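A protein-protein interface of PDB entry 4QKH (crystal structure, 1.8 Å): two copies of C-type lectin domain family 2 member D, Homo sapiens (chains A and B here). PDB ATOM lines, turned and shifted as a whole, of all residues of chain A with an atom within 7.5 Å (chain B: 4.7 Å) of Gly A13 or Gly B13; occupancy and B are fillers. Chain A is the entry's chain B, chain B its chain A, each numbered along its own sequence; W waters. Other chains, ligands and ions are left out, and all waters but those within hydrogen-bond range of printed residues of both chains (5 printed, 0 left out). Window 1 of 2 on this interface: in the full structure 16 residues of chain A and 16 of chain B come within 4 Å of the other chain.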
ATOM      1  N   ALA A   6      -5.655  18.862  -7.607  1.00  0.00           N
ATOM      2  CA  ALA A   6      -5.025  18.477  -8.850  1.00  0.00           C
ATOM      3  C   ALA A   6      -5.158  16.954  -9.005  1.00  0.00           C
ATOM      4  O   ALA A   6      -5.266  16.469 -10.136  1.00  0.00           O
ATOM      5  CB  ALA A   6      -3.552  18.904  -8.870  1.00  0.00           C
ATOM      6  N   CYS A   7      -5.174  16.234  -7.881  1.00  0.00           N
ATOM      7  CA  CYS A   7      -5.088  14.764  -7.835  1.00  0.00           C
ATOM      8  C   CYS A   7      -6.227  14.187  -7.021  1.00  0.00           C
ATOM      9  O   CYS A   7      -6.729  14.848  -6.122  1.00  0.00           O
ATOM     10  CB  CYS A   7      -3.729  14.299  -7.210  1.00  0.00           C
ATOM     11  SG  CYS A   7      -2.316  14.764  -8.211  1.00  0.00           S
ATOM     12  N   PRO A   8      -6.672  12.968  -7.341  1.00  0.00           N
ATOM     13  CA  PRO A   8      -7.695  12.321  -6.506  1.00  0.00           C
ATOM     14  C   PRO A   8      -7.266  12.076  -5.060  1.00  0.00           C
ATOM     15  O   PRO A   8      -6.051  12.103  -4.777  1.00  0.00           O
ATOM     16  CB  PRO A   8      -7.949  10.980  -7.221  1.00  0.00           C
ATOM     17  CG  PRO A   8      -7.251  11.034  -8.475  1.00  0.00           C
ATOM     18  CD  PRO A   8      -6.198  12.082  -8.416  1.00  0.00           C
ATOM     19  N   SER A  10      -5.929  10.638  -1.725  1.00  0.00           N
ATOM     20  CA  SER A  10      -4.892   9.665  -1.392  1.00  0.00           C
ATOM     21  C   SER A  10      -3.913   9.345  -2.541  1.00  0.00           C
ATOM     22  O   SER A  10      -3.065   8.438  -2.403  1.00  0.00           O
ATOM     23  CB  SER A  10      -5.485   8.378  -0.773  1.00  0.00           C
ATOM     24  OG  SER A  10      -5.750   7.363  -1.739  1.00  0.00           O
ATOM     25  N   TRP A  11      -3.983  10.070  -3.655  1.00  0.00           N
ATOM     26  CA  TRP A  11      -2.976   9.943  -4.657  1.00  0.00           C
ATOM     27  C   TRP A  11      -1.842  10.957  -4.403  1.00  0.00           C
ATOM     28  O   TRP A  11      -2.022  11.929  -3.650  1.00  0.00           O
ATOM     29  CB  TRP A  11      -3.537  10.112  -6.042  1.00  0.00           C
ATOM     30  CG  TRP A  11      -4.549   9.054  -6.505  1.00  0.00           C
ATOM     31  CD1 TRP A  11      -5.569   8.488  -5.775  1.00  0.00           C
ATOM     32  CD2 TRP A  11      -4.632   8.502  -7.819  1.00  0.00           C
ATOM     33  NE1 TRP A  11      -6.256   7.590  -6.576  1.00  0.00           N
ATOM     34  CE2 TRP A  11      -5.712   7.600  -7.823  1.00  0.00           C
ATOM     35  CE3 TRP A  11      -3.880   8.675  -9.009  1.00  0.00           C
ATOM     36  CZ2 TRP A  11      -6.047   6.861  -8.935  1.00  0.00           C
ATOM     37  CZ3 TRP A  11      -4.216   7.974 -10.111  1.00  0.00           C
ATOM     38  CH2 TRP A  11      -5.304   7.064 -10.084  1.00  0.00           C
ATOM     39  N   ILE A  12      -0.691  10.691  -5.010  1.00  0.00           N
ATOM     40  CA  ILE A  12       0.558  11.434  -4.716  1.00  0.00           C
ATOM     41  C   ILE A  12       0.899  12.261  -5.954  1.00  0.00           C
ATOM     42  O   ILE A  12       0.926  11.753  -7.115  1.00  0.00           O
ATOM     43  CB  ILE A  12       1.792  10.494  -4.408  1.00  0.00           C
ATOM     44  CG1 ILE A  12       1.533   9.373  -3.371  1.00  0.00           C
ATOM     45  CG2 ILE A  12       3.040  11.347  -4.082  1.00  0.00           C
ATOM     46  CD1 ILE A  12       0.906   9.741  -2.071  1.00  0.00           C
ATOM     47  N   GLY A  13       1.130  13.574  -5.711  1.00  0.00           N
ATOM     48  CA  GLY A  13       1.343  14.541  -6.741  1.00  0.00           C
ATOM     49  C   GLY A  13       2.820  14.754  -6.987  1.00  0.00           C
ATOM     50  O   GLY A  13       3.575  14.966  -6.047  1.00  0.00           O
ATOM     51  N   PHE A  14       3.228  14.583  -8.222  1.00  0.00           N
ATOM     52  CA  PHE A  14       4.591  14.905  -8.680  1.00  0.00           C
ATOM     53  C   PHE A  14       4.512  15.624 -10.026  1.00  0.00           C
ATOM     54  O   PHE A  14       4.026  15.034 -11.000  1.00  0.00           O
ATOM     55  CB  PHE A  14       5.413  13.631  -8.809  1.00  0.00           C
ATOM     56  CG  PHE A  14       6.874  13.867  -9.172  1.00  0.00           C
ATOM     57  CD1 PHE A  14       7.788  14.257  -8.211  1.00  0.00           C
ATOM     58  CD2 PHE A  14       7.342  13.612 -10.435  1.00  0.00           C
ATOM     59  CE1 PHE A  14       9.118  14.482  -8.532  1.00  0.00           C
ATOM     60  CE2 PHE A  14       8.695  13.813 -10.765  1.00  0.00           C
ATOM     61  CZ  PHE A  14       9.578  14.270  -9.798  1.00  0.00           C
ATOM     62  N   GLN A  15       5.056  16.842 -10.098  1.00  0.00           N
ATOM     63  CA  GLN A  15       5.035  17.689 -11.306  1.00  0.00           C
ATOM     64  C   GLN A  15       3.569  17.845 -11.789  1.00  0.00           C
ATOM     65  O   GLN A  15       2.732  18.290 -10.997  1.00  0.00           O
ATOM     66  CB  GLN A  15       6.040  17.177 -12.356  1.00  0.00           C
ATOM     67  CG  GLN A  15       7.468  17.261 -11.852  1.00  0.00           C
ATOM     68  CD  GLN A  15       8.528  16.774 -12.834  1.00  0.00           C
ATOM     69  OE1 GLN A  15       8.330  15.845 -13.607  1.00  0.00           O
ATOM     70  NE2 GLN A  15       9.683  17.400 -12.774  1.00  0.00           N
ATOM     71  N   ARG A  16       3.253  17.461 -13.029  1.00  0.00           N
ATOM     72  CA  ARG A  16       1.880  17.606 -13.566  1.00  0.00           C
ATOM     73  C   ARG A  16       1.166  16.255 -13.622  1.00  0.00           C
ATOM     74  O   ARG A  16       0.199  16.067 -14.377  1.00  0.00           O
ATOM     75  CB  ARG A  16       1.904  18.230 -14.979  1.00  0.00           C
ATOM     76  CG  ARG A  16       2.524  19.644 -15.048  1.00  0.00           C
ATOM     77  CD  ARG A  16       1.911  20.638 -14.080  1.00  0.00           C
ATOM     78  NE  ARG A  16       0.463  20.809 -14.225  1.00  0.00           N
ATOM     79  CZ  ARG A  16      -0.138  21.674 -15.045  1.00  0.00           C
ATOM     80  NH1 ARG A  16       0.577  22.468 -15.831  1.00  0.00           N
ATOM     81  NH2 ARG A  16      -1.472  21.733 -15.078  1.00  0.00           N
ATOM     82  N   LYS A  17       1.618  15.316 -12.801  1.00  0.00           N
ATOM     83  CA  LYS A  17       1.024  13.992 -12.742  1.00  0.00           C
ATOM     84  C   LYS A  17       0.584  13.582 -11.341  1.00  0.00           C
ATOM     85  O   LYS A  17       1.017  14.193 -10.332  1.00  0.00           O
ATOM     86  CB  LYS A  17       2.015  12.992 -13.284  1.00  0.00           C
ATOM     87  CG  LYS A  17       2.101  13.042 -14.784  1.00  0.00           C
ATOM     88  CD  LYS A  17       3.366  12.369 -15.263  1.00  0.00           C
ATOM     89  CE  LYS A  17       3.091  11.245 -16.228  1.00  0.00           C
ATOM     90  NZ  LYS A  17       4.336  10.774 -16.884  1.00  0.00           N
ATOM     91  N   CYS A  18      -0.300  12.576 -11.277  1.00  0.00           N
ATOM     92  CA  CYS A  18      -0.864  12.027 -10.040  1.00  0.00           C
ATOM     93  C   CYS A  18      -0.664  10.514 -10.052  1.00  0.00           C
ATOM     94  O   CYS A  18      -0.906   9.871 -11.062  1.00  0.00           O
ATOM     95  CB  CYS A  18      -2.386  12.289  -9.871  1.00  0.00           C
ATOM     96  SG  CYS A  18      -2.748  14.075 -10.115  1.00  0.00           S
ATOM     97  N   PHE A  19      -0.236   9.984  -8.926  1.00  0.00           N
ATOM     98  CA  PHE A  19       0.158   8.556  -8.825  1.00  0.00           C
ATOM     99  C   PHE A  19      -0.551   7.834  -7.698  1.00  0.00           C
ATOM    100  O   PHE A  19      -0.759   8.365  -6.565  1.00  0.00           O
ATOM    101  CB  PHE A  19       1.661   8.420  -8.641  1.00  0.00           C
ATOM    102  CG  PHE A  19       2.473   8.949  -9.771  1.00  0.00           C
ATOM    103  CD1 PHE A  19       2.861  10.270  -9.789  1.00  0.00           C
ATOM    104  CD2 PHE A  19       2.811   8.137 -10.833  1.00  0.00           C
ATOM    105  CE1 PHE A  19       3.661  10.745 -10.832  1.00  0.00           C
ATOM    106  CE2 PHE A  19       3.587   8.600 -11.904  1.00  0.00           C
ATOM    107  CZ  PHE A  19       4.004   9.926 -11.892  1.00  0.00           C
ATOM    108  N   PHE A  53      11.543   9.308  -8.323  1.00  0.00           N
ATOM    109  CA  PHE A  53      10.454   9.615  -7.428  1.00  0.00           C
ATOM    110  C   PHE A  53       9.685   8.303  -7.056  1.00  0.00           C
ATOM    111  O   PHE A  53       9.434   7.985  -5.906  1.00  0.00           O
ATOM    112  CB  PHE A  53       9.499  10.642  -8.073  1.00  0.00           C
ATOM    113  CG  PHE A  53       8.111  10.598  -7.493  1.00  0.00           C
ATOM    114  CD1 PHE A  53       7.909  11.024  -6.187  1.00  0.00           C
ATOM    115  CD2 PHE A  53       7.037  10.088  -8.201  1.00  0.00           C
ATOM    116  CE1 PHE A  53       6.644  10.933  -5.611  1.00  0.00           C
ATOM    117  CE2 PHE A  53       5.756  10.019  -7.638  1.00  0.00           C
ATOM    118  CZ  PHE A  53       5.568  10.437  -6.350  1.00  0.00           C
ATOM    119  N   ASP A 120      -2.681  15.685 -13.955  1.00  0.00           N
ATOM    120  CA  ASP A 120      -3.514  16.363 -12.987  1.00  0.00           C
ATOM    121  C   ASP A 120      -4.661  17.041 -13.767  1.00  0.00           C
ATOM    122  O   ASP A 120      -4.572  17.257 -14.956  1.00  0.00           O
ATOM    123  CB  ASP A 120      -2.758  17.363 -12.117  1.00  0.00           C
ATOM    124  CG  ASP A 120      -2.306  18.596 -12.869  1.00  0.00           C
ATOM    125  OD1 ASP A 120      -3.110  19.222 -13.633  1.00  0.00           O
ATOM    126  OD2 ASP A 120      -1.134  18.976 -12.682  1.00  0.00           O
ATOM    127  N   CYS B   7       2.301  22.076  -6.876  1.00  0.00           N
ATOM    128  CA  CYS B   7       3.445  22.238  -5.983  1.00  0.00           C
ATOM    129  C   CYS B   7       4.674  22.756  -6.718  1.00  0.00           C
ATOM    130  O   CYS B   7       4.832  22.495  -7.899  1.00  0.00           O
ATOM    131  CB  CYS B   7       3.725  20.872  -5.281  1.00  0.00           C
ATOM    132  SG  CYS B   7       2.412  20.233  -4.226  1.00  0.00           S
ATOM    133  N   TRP B  11       8.987  19.453  -4.816  1.00  0.00           N
ATOM    134  CA  TRP B  11       8.076  19.228  -3.727  1.00  0.00           C
ATOM    135  C   TRP B  11       7.077  18.173  -4.155  1.00  0.00           C
ATOM    136  O   TRP B  11       6.722  18.092  -5.335  1.00  0.00           O
ATOM    137  CB  TRP B  11       7.317  20.492  -3.344  1.00  0.00           C
ATOM    138  CG  TRP B  11       8.198  21.614  -2.780  1.00  0.00           C
ATOM    139  CD1 TRP B  11       9.276  22.172  -3.367  1.00  0.00           C
ATOM    140  CD2 TRP B  11       8.038  22.275  -1.537  1.00  0.00           C
ATOM    141  NE1 TRP B  11       9.778  23.192  -2.571  1.00  0.00           N
ATOM    142  CE2 TRP B  11       9.021  23.254  -1.446  1.00  0.00           C
ATOM    143  CE3 TRP B  11       7.131  22.126  -0.477  1.00  0.00           C
ATOM    144  CZ2 TRP B  11       9.202  24.032  -0.298  1.00  0.00           C
ATOM    145  CZ3 TRP B  11       7.280  22.968   0.657  1.00  0.00           C
ATOM    146  CH2 TRP B  11       8.282  23.926   0.684  1.00  0.00           C
ATOM    147  N   ILE B  12       6.554  17.437  -3.187  1.00  0.00           N
ATOM    148  CA  ILE B  12       5.685  16.297  -3.405  1.00  0.00           C
ATOM    149  C   ILE B  12       4.309  16.638  -2.849  1.00  0.00           C
ATOM    150  O   ILE B  12       4.201  17.162  -1.717  1.00  0.00           O
ATOM    151  CB  ILE B  12       6.207  15.048  -2.646  1.00  0.00           C
ATOM    152  CG1 ILE B  12       7.671  14.754  -3.036  1.00  0.00           C
ATOM    153  CG2 ILE B  12       5.300  13.869  -2.886  1.00  0.00           C
ATOM    154  CD1 ILE B  12       8.033  14.772  -4.475  1.00  0.00           C
ATOM    155  N   GLY B  13       3.278  16.293  -3.615  1.00  0.00           N
ATOM    156  CA  GLY B  13       1.896  16.590  -3.244  1.00  0.00           C
ATOM    157  C   GLY B  13       1.176  15.503  -2.565  1.00  0.00           C
ATOM    158  O   GLY B  13       1.251  14.338  -2.988  1.00  0.00           O
ATOM    159  N   PHE B  14       0.484  15.821  -1.477  1.00  0.00           N
ATOM    160  CA  PHE B  14      -0.295  14.841  -0.777  1.00  0.00           C
ATOM    161  C   PHE B  14      -1.405  15.535   0.027  1.00  0.00           C
ATOM    162  O   PHE B  14      -1.144  16.436   0.817  1.00  0.00           O
ATOM    163  CB  PHE B  14       0.594  13.978   0.119  1.00  0.00           C
ATOM    164  CG  PHE B  14      -0.147  12.895   0.850  1.00  0.00           C
ATOM    165  CD1 PHE B  14      -0.493  11.740   0.190  1.00  0.00           C
ATOM    166  CD2 PHE B  14      -0.516  13.044   2.157  1.00  0.00           C
ATOM    167  CE1 PHE B  14      -1.185  10.741   0.822  1.00  0.00           C
ATOM    168  CE2 PHE B  14      -1.202  12.039   2.806  1.00  0.00           C
ATOM    169  CZ  PHE B  14      -1.525  10.879   2.134  1.00  0.00           C
ATOM    170  N   GLN B  15      -2.653  15.123  -0.194  1.00  0.00           N
ATOM    171  CA  GLN B  15      -3.795  15.694   0.540  1.00  0.00           C
ATOM    172  C   GLN B  15      -3.837  17.225   0.633  1.00  0.00           C
ATOM    173  O   GLN B  15      -3.995  17.777   1.727  1.00  0.00           O
ATOM    174  CB  GLN B  15      -3.841  15.131   1.957  1.00  0.00           C
ATOM    175  CG  GLN B  15      -4.258  13.676   2.035  1.00  0.00           C
ATOM    176  CD  GLN B  15      -4.448  13.217   3.481  1.00  0.00           C
ATOM    177  OE1 GLN B  15      -4.104  13.939   4.425  1.00  0.00           O
ATOM    178  NE2 GLN B  15      -4.999  12.013   3.662  1.00  0.00           N
ATOM    179  N   LYS B  17      -1.511  19.407   0.184  1.00  0.00           N
ATOM    180  CA  LYS B  17      -0.281  20.033   0.584  1.00  0.00           C
ATOM    181  C   LYS B  17       0.864  19.601  -0.241  1.00  0.00           C
ATOM    182  O   LYS B  17       0.757  18.655  -0.999  1.00  0.00           O
ATOM    183  CB  LYS B  17       0.021  19.701   2.038  1.00  0.00           C
ATOM    184  CG  LYS B  17      -0.836  20.471   3.001  1.00  0.00           C
ATOM    185  CD  LYS B  17      -1.258  19.647   4.166  1.00  0.00           C
ATOM    186  CE  LYS B  17      -0.227  19.482   5.240  1.00  0.00           C
ATOM    187  NZ  LYS B  17      -0.877  18.909   6.464  1.00  0.00           N
ATOM    188  N   CYS B  18       1.954  20.352  -0.098  1.00  0.00           N
ATOM    189  CA  CYS B  18       3.182  20.167  -0.801  1.00  0.00           C
ATOM    190  C   CYS B  18       4.261  19.987   0.253  1.00  0.00           C
ATOM    191  O   CYS B  18       4.348  20.822   1.203  1.00  0.00           O
ATOM    192  CB  CYS B  18       3.470  21.409  -1.579  1.00  0.00           C
ATOM    193  SG  CYS B  18       2.215  21.797  -2.879  1.00  0.00           S
HETATM  194  O   HOH W   1       3.076  19.480  -8.590  1.00  0.00           O
HETATM  195  O   HOH W   2      -3.702  13.315  -2.182  1.00  0.00           O
HETATM  196  O   HOH W   3       4.321  17.686  -6.748  1.00  0.00           O
HETATM  197  O   HOH W   4      -1.800  14.871  -4.373  1.00  0.00           O
HETATM  198  O   HOH W   5       6.985  18.028  -8.146  1.00  0.00           O
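N of Gly B13 lies within hydrogen-bond range of O of Gly A13 (2.8 Å).
The backbone carbonyl oxygen (O) of Ile A12 lies within hydrogen-bond range of the backbone NH (N) of Phe A19, 2.8 Å away. The side-chain sulfur (SG) of Cys B7 is disulfide-bonded to the side-chain sulfur (SG) of Cys B18 (2.1 Å). The side-chain sulfur (SG) of Cys A18 forms a disulfide with the side-chain sulfur (SG) of Cys A7.
Ile A12 touches Ile B12 (CG2 to CG2, 3.6 Å). CA of Ile A12 touches O of Gly B13, 3.4 Å away. CD1 of Phe B14 touches CD1 of Ile A12, at 3.3 Å. Ile B12 touches Gly A13 (CA to O, 3.6 Å). CD1 of Ile B12 touches CD1 of Phe A14 (3.8 Å).
Pro A8 touches none of the printed residues of chain B. Of the printed residues of chain B, Ile A12 touches Ile B12 (3.6 Å), Gly B13 (3.4 Å) and Phe B14 (3.3 Å). Of chain B, only Ile B12 (3.6 Å) and Gly B13 (2.8 Å) come within 4 Å of Gly A13. Of the printed residues of chain B, Phe A14 touches Ile B12. Of chain A, only Ile A12 and Gly A13 come within 4 Å of Gly B13. Of the printed residues of chain A, Phe B14 touches Ile A12 (3.3 Å). The nearest residue of chain A that does not touch Gly B13 is Trp A11 (4.1 Å).
Hydrophobic or aromatic side chains of chain B that line the printed part of chain A: Ile B12 and Phe B14. Of the 15 printed residues of chain A, 3 touch a printed residue of chain B. Printed residues of chain A that touch a printed residue of chain B: Ile A12, Gly A13 and Phe A14.
Ile B12 touches its own counterpart, Ile A12. Ile A12 touches Gly B13, and with the chains exchanged Gly A13 touches Ile B12. Ile A12 touches Phe B14, and with the chains exchanged Phe A14 touches Ile B12. Gly A13 touches its own counterpart, Gly B13. Of the 6 pairs that touch across the chains among the printed residues, 6 have their exchanged pair printed and touching as well.
Water W2 bridges O of Trp A11 (2.6 Å) and N of Gln B15 (2.9 Å). Water W1 lies within hydrogen-bond range of the backbone carbonyl oxygen (O) of Gln A15 (2.7 Å) and the backbone NH (N) of Cys B7 (3.2 Å). Water W3 bridges the backbone carbonyl oxygen of Trp B11 (2.8 Å) and the backbone carbonyl oxygen of Gly A13 (2.9 Å). Water W5 bridges O of Trp B11 (2.8 Å) and N of Gln A15 (3.0 Å). Water W4 lies within hydrogen-bond range of O of Trp A11, O of Gly B13 and N of Gly A13.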
